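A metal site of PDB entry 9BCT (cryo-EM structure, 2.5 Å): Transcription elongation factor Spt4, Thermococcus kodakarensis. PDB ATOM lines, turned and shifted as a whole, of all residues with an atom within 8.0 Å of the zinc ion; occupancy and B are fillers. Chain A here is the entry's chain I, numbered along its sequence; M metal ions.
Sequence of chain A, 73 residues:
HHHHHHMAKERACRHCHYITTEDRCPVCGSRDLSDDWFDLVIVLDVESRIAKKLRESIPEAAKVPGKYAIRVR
Four residues have an atom within 4 Å of the zinc ion: Cys 13, Cys 16, Cys 25 and Cys 28.
Along chain A the residues within 4 Å of the zinc ion span positions 13 to 28.
The nearest printed residue that does not touch the zinc ion is Tyr 18 (4.7 Å).
The backbone NH (N) of Ser 30 sits close to the side-chain sulfur (SG) of Cys 28 (3.4 Å).
N of Tyr 18 sits close to SG of Cys 16, 3.7 Å away.
The backbone NH (N) of Cys 13 is in hydrogen-bond range of the backbone carbonyl oxygen (O) of Tyr 18, at 2.7 Å.
The backbone NH of His 15 sits close to the side-chain sulfur of Cys 13 (3.4 Å).
The zinc ion is bound by SG of Cys 28, SG of Cys 16, SG of Cys 13 and SG of Cys 25.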
ATOM      1  N   ALA A  12      31.729  13.928  28.228  1.00  0.00           N
ATOM      2  CA  ALA A  12      30.320  14.257  28.385  1.00  0.00           C
ATOM      3  C   ALA A  12      30.058  15.676  27.876  1.00  0.00           C
ATOM      4  O   ALA A  12      30.879  16.570  28.082  1.00  0.00           O
ATOM      5  CB  ALA A  12      29.874  14.148  29.845  1.00  0.00           C
ATOM      6  N   CYS A  13      28.921  15.856  27.215  1.00  0.00           N
ATOM      7  CA  CYS A  13      28.553  17.160  26.698  1.00  0.00           C
ATOM      8  C   CYS A  13      28.176  18.103  27.837  1.00  0.00           C
ATOM      9  O   CYS A  13      27.792  17.683  28.924  1.00  0.00           O
ATOM     10  CB  CYS A  13      27.392  17.031  25.710  1.00  0.00           C
ATOM     11  SG  CYS A  13      26.826  18.590  25.000  1.00  0.00           S
ATOM     12  N   ARG A  14      28.305  19.401  27.560  1.00  0.00           N
ATOM     13  CA  ARG A  14      28.014  20.421  28.565  1.00  0.00           C
ATOM     14  C   ARG A  14      26.630  21.038  28.417  1.00  0.00           C
ATOM     15  O   ARG A  14      26.088  21.552  29.407  1.00  0.00           O
ATOM     16  CB  ARG A  14      29.059  21.537  28.508  1.00  0.00           C
ATOM     17  CG  ARG A  14      29.296  22.235  29.835  1.00  0.00           C
ATOM     18  CD  ARG A  14      30.431  23.247  29.746  1.00  0.00           C
ATOM     19  NE  ARG A  14      31.715  22.656  30.129  1.00  0.00           N
ATOM     20  CZ  ARG A  14      32.616  22.207  29.275  1.00  0.00           C
ATOM     21  NH1 ARG A  14      32.416  22.242  27.963  1.00  0.00           N
ATOM     22  NH2 ARG A  14      33.759  21.700  29.740  1.00  0.00           N
ATOM     23  N   HIS A  15      26.030  21.000  27.226  1.00  0.00           N
ATOM     24  CA  HIS A  15      24.721  21.598  27.007  1.00  0.00           C
ATOM     25  C   HIS A  15      23.595  20.629  27.364  1.00  0.00           C
ATOM     26  O   HIS A  15      22.786  20.907  28.248  1.00  0.00           O
ATOM     27  CB  HIS A  15      24.592  22.063  25.547  1.00  0.00           C
ATOM     28  CG  HIS A  15      23.223  22.559  25.196  1.00  0.00           C
ATOM     29  ND1 HIS A  15      22.574  22.184  24.048  1.00  0.00           N
ATOM     30  CD2 HIS A  15      22.394  23.411  25.841  1.00  0.00           C
ATOM     31  CE1 HIS A  15      21.392  22.769  23.992  1.00  0.00           C
ATOM     32  NE2 HIS A  15      21.261  23.519  25.075  1.00  0.00           N
ATOM     33  N   CYS A  16      23.542  19.483  26.688  1.00  0.00           N
ATOM     34  CA  CYS A  16      22.514  18.480  26.933  1.00  0.00           C
ATOM     35  C   CYS A  16      22.946  17.418  27.933  1.00  0.00           C
ATOM     36  O   CYS A  16      22.156  16.527  28.239  1.00  0.00           O
ATOM     37  CB  CYS A  16      22.107  17.808  25.619  1.00  0.00           C
ATOM     38  SG  CYS A  16      23.416  16.847  24.843  1.00  0.00           S
ATOM     39  N   HIS A  17      24.190  17.493  28.432  1.00  0.00           N
ATOM     40  CA  HIS A  17      24.709  16.583  29.453  1.00  0.00           C
ATOM     41  C   HIS A  17      24.693  15.127  28.993  1.00  0.00           C
ATOM     42  O   HIS A  17      24.514  14.216  29.805  1.00  0.00           O
ATOM     43  CB  HIS A  17      23.963  16.736  30.780  1.00  0.00           C
ATOM     44  CG  HIS A  17      24.121  18.078  31.422  1.00  0.00           C
ATOM     45  ND1 HIS A  17      24.268  18.241  32.778  1.00  0.00           N
ATOM     46  CD2 HIS A  17      24.132  19.330  30.889  1.00  0.00           C
ATOM     47  CE1 HIS A  17      24.378  19.531  33.061  1.00  0.00           C
ATOM     48  NE2 HIS A  17      24.306  20.208  31.934  1.00  0.00           N
ATOM     49  N   TYR A  18      24.873  14.896  27.693  1.00  0.00           N
ATOM     50  CA  TYR A  18      24.888  13.550  27.152  1.00  0.00           C
ATOM     51  C   TYR A  18      26.283  12.956  27.238  1.00  0.00           C
ATOM     52  O   TYR A  18      27.281  13.669  27.103  1.00  0.00           O
ATOM     53  CB  TYR A  18      24.416  13.557  25.693  1.00  0.00           C
ATOM     54  CG  TYR A  18      23.995  12.198  25.170  1.00  0.00           C
ATOM     55  CD1 TYR A  18      22.714  11.711  25.387  1.00  0.00           C
ATOM     56  CD2 TYR A  18      24.883  11.418  24.437  1.00  0.00           C
ATOM     57  CE1 TYR A  18      22.327  10.473  24.901  1.00  0.00           C
ATOM     58  CE2 TYR A  18      24.504  10.181  23.956  1.00  0.00           C
ATOM     59  CZ  TYR A  18      23.230   9.716  24.181  1.00  0.00           C
ATOM     60  OH  TYR A  18      22.846   8.482  23.708  1.00  0.00           O
ATOM     61  N   ILE A  19      26.350  11.643  27.476  1.00  0.00           N
ATOM     62  CA  ILE A  19      27.606  10.918  27.553  1.00  0.00           C
ATOM     63  C   ILE A  19      27.820  10.198  26.240  1.00  0.00           C
ATOM     64  O   ILE A  19      26.989   9.371  25.824  1.00  0.00           O
ATOM     65  CB  ILE A  19      27.609   9.931  28.738  1.00  0.00           C
ATOM     66  CG1 ILE A  19      27.731  10.685  30.063  1.00  0.00           C
ATOM     67  CG2 ILE A  19      28.736   8.918  28.588  1.00  0.00           C
ATOM     68  CD1 ILE A  19      26.432  10.814  30.826  1.00  0.00           C
ATOM     69  N   THR A  20      28.930  10.505  25.565  1.00  0.00           N
ATOM     70  CA  THR A  20      29.224   9.915  24.265  1.00  0.00           C
ATOM     71  C   THR A  20      30.692   9.498  24.234  1.00  0.00           C
ATOM     72  O   THR A  20      31.528  10.009  24.983  1.00  0.00           O
ATOM     73  CB  THR A  20      28.934  10.897  23.121  1.00  0.00           C
ATOM     74  OG1 THR A  20      29.241  10.275  21.863  1.00  0.00           O
ATOM     75  CG2 THR A  20      29.755  12.162  23.268  1.00  0.00           C
ATOM     76  N   ARG A  24      31.717  13.842  18.213  1.00  0.00           N
ATOM     77  CA  ARG A  24      30.438  14.430  17.821  1.00  0.00           C
ATOM     78  C   ARG A  24      29.374  14.172  18.880  1.00  0.00           C
ATOM     79  O   ARG A  24      29.323  13.106  19.495  1.00  0.00           O
ATOM     80  CB  ARG A  24      29.991  13.867  16.470  1.00  0.00           C
ATOM     81  CG  ARG A  24      28.773  14.554  15.861  1.00  0.00           C
ATOM     82  CD  ARG A  24      29.107  15.949  15.318  1.00  0.00           C
ATOM     83  NE  ARG A  24      29.032  16.980  16.347  1.00  0.00           N
ATOM     84  CZ  ARG A  24      27.948  17.712  16.597  1.00  0.00           C
ATOM     85  NH1 ARG A  24      26.828  17.541  15.925  1.00  0.00           N
ATOM     86  NH2 ARG A  24      27.997  18.634  17.555  1.00  0.00           N
ATOM     87  N   CYS A  25      28.510  15.169  19.091  1.00  0.00           N
ATOM     88  CA  CYS A  25      27.353  15.007  19.966  1.00  0.00           C
ATOM     89  C   CYS A  25      26.128  14.825  19.093  1.00  0.00           C
ATOM     90  O   CYS A  25      25.693  15.799  18.448  1.00  0.00           O
ATOM     91  CB  CYS A  25      27.196  16.207  20.887  1.00  0.00           C
ATOM     92  SG  CYS A  25      26.072  15.945  22.276  1.00  0.00           S
ATOM     93  N   PRO A  26      25.540  13.634  19.018  1.00  0.00           N
ATOM     94  CA  PRO A  26      24.489  13.386  18.027  1.00  0.00           C
ATOM     95  C   PRO A  26      23.084  13.719  18.499  1.00  0.00           C
ATOM     96  O   PRO A  26      22.106  13.313  17.873  1.00  0.00           O
ATOM     97  CB  PRO A  26      24.635  11.887  17.749  1.00  0.00           C
ATOM     98  CG  PRO A  26      25.130  11.322  19.057  1.00  0.00           C
ATOM     99  CD  PRO A  26      25.865  12.428  19.790  1.00  0.00           C
ATOM    100  N   VAL A  27      22.963  14.453  19.606  1.00  0.00           N
ATOM    101  CA  VAL A  27      21.666  14.774  20.193  1.00  0.00           C
ATOM    102  C   VAL A  27      21.388  16.273  20.154  1.00  0.00           C
ATOM    103  O   VAL A  27      20.293  16.693  19.771  1.00  0.00           O
ATOM    104  CB  VAL A  27      21.567  14.228  21.634  1.00  0.00           C
ATOM    105  CG1 VAL A  27      20.233  14.606  22.264  1.00  0.00           C
ATOM    106  CG2 VAL A  27      21.746  12.721  21.644  1.00  0.00           C
ATOM    107  N   CYS A  28      22.365  17.093  20.537  1.00  0.00           N
ATOM    108  CA  CYS A  28      22.183  18.535  20.597  1.00  0.00           C
ATOM    109  C   CYS A  28      22.954  19.301  19.539  1.00  0.00           C
ATOM    110  O   CYS A  28      22.615  20.450  19.262  1.00  0.00           O
ATOM    111  CB  CYS A  28      22.573  19.064  21.988  1.00  0.00           C
ATOM    112  SG  CYS A  28      24.342  19.295  22.203  1.00  0.00           S
ATOM    113  N   GLY A  29      23.973  18.687  18.932  1.00  0.00           N
ATOM    114  CA  GLY A  29      24.751  19.368  17.908  1.00  0.00           C
ATOM    115  C   GLY A  29      25.573  20.542  18.402  1.00  0.00           C
ATOM    116  O   GLY A  29      25.611  21.583  17.729  1.00  0.00           O
ATOM    117  N   SER A  30      26.229  20.401  19.544  1.00  0.00           N
ATOM    118  CA  SER A  30      27.119  21.428  20.068  1.00  0.00           C
ATOM    119  C   SER A  30      28.549  20.921  20.108  1.00  0.00           C
ATOM    120  O   SER A  30      28.810  19.713  20.059  1.00  0.00           O
ATOM    121  CB  SER A  30      26.671  21.877  21.463  1.00  0.00           C
ATOM    122  OG  SER A  30      27.447  22.973  21.921  1.00  0.00           O
ATOM    123  N   ARG A  31      29.492  21.862  20.199  1.00  0.00           N
ATOM    124  CA  ARG A  31      30.915  21.568  20.098  1.00  0.00           C
ATOM    125  C   ARG A  31      31.658  21.758  21.414  1.00  0.00           C
ATOM    126  O   ARG A  31      32.850  22.069  21.425  1.00  0.00           O
ATOM    127  CB  ARG A  31      31.555  22.425  19.004  1.00  0.00           C
ATOM    128  CG  ARG A  31      30.849  22.347  17.658  1.00  0.00           C
ATOM    129  CD  ARG A  31      30.631  20.909  17.208  1.00  0.00           C
ATOM    130  NE  ARG A  31      31.888  20.199  17.038  1.00  0.00           N
ATOM    131  CZ  ARG A  31      32.195  19.066  17.653  1.00  0.00           C
ATOM    132  NH1 ARG A  31      31.342  18.475  18.480  1.00  0.00           N
ATOM    133  NH2 ARG A  31      33.367  18.495  17.421  1.00  0.00           N
ATOM    134  N   ASP A  32      30.969  21.586  22.539  1.00  0.00           N
ATOM    135  CA  ASP A  32      31.588  21.677  23.855  1.00  0.00           C
ATOM    136  C   ASP A  32      31.542  20.310  24.518  1.00  0.00           C
ATOM    137  O   ASP A  32      30.476  19.708  24.647  1.00  0.00           O
ATOM    138  CB  ASP A  32      30.884  22.715  24.736  1.00  0.00           C
ATOM    139  CG  ASP A  32      29.390  22.759  24.509  1.00  0.00           C
ATOM    140  OD1 ASP A  32      28.873  21.880  23.785  1.00  0.00           O
ATOM    141  OD2 ASP A  32      28.727  23.668  25.060  1.00  0.00           O
ATOM    142  N   LEU A  33      32.713  19.817  24.935  1.00  0.00           N
ATOM    143  CA  LEU A  33      32.829  18.493  25.531  1.00  0.00           C
ATOM    144  C   LEU A  33      33.698  18.584  26.774  1.00  0.00           C
ATOM    145  O   LEU A  33      34.726  19.263  26.789  1.00  0.00           O
ATOM    146  CB  LEU A  33      33.437  17.488  24.535  1.00  0.00           C
ATOM    147  CG  LEU A  33      32.708  16.159  24.391  1.00  0.00           C
ATOM    148  CD1 LEU A  33      31.219  16.381  24.166  1.00  0.00           C
ATOM    149  CD2 LEU A  33      33.305  15.347  23.261  1.00  0.00           C
ATOM    150  N   GLU A  60      16.911  20.490  27.924  1.00  0.00           N
ATOM    151  CA  GLU A  60      17.469  19.889  26.708  1.00  0.00           C
ATOM    152  C   GLU A  60      18.069  18.513  26.962  1.00  0.00           C
ATOM    153  O   GLU A  60      18.872  18.028  26.160  1.00  0.00           O
ATOM    154  CB  GLU A  60      18.524  20.817  26.095  1.00  0.00           C
ATOM    155  CG  GLU A  60      19.773  21.082  26.940  1.00  0.00           C
ATOM    156  CD  GLU A  60      19.561  22.101  28.050  1.00  0.00           C
ATOM    157  OE1 GLU A  60      18.428  22.247  28.540  1.00  0.00           O
ATOM    158  OE2 GLU A  60      20.551  22.763  28.437  1.00  0.00           O
ATOM    159  N   TYR A  68      22.889  10.311  30.551  1.00  0.00           N
ATOM    160  CA  TYR A  68      22.766  11.725  30.873  1.00  0.00           C
ATOM    161  C   TYR A  68      23.372  11.980  32.245  1.00  0.00           C
ATOM    162  O   TYR A  68      23.815  11.060  32.935  1.00  0.00           O
ATOM    163  CB  TYR A  68      21.300  12.180  30.819  1.00  0.00           C
ATOM    164  CG  TYR A  68      20.713  12.224  29.438  1.00  0.00           C
ATOM    165  CD1 TYR A  68      20.905  13.328  28.613  1.00  0.00           C
ATOM    166  CD2 TYR A  68      19.958  11.166  28.941  1.00  0.00           C
ATOM    167  CE1 TYR A  68      20.372  13.364  27.339  1.00  0.00           C
ATOM    168  CE2 TYR A  68      19.420  11.195  27.678  1.00  0.00           C
ATOM    169  CZ  TYR A  68      19.624  12.303  26.871  1.00  0.00           C
ATOM    170  OH  TYR A  68      19.087  12.341  25.605  1.00  0.00           O
HETATM  171 ZN    ZN M   1      25.211  17.660  23.599  1.00  0.00          ZN
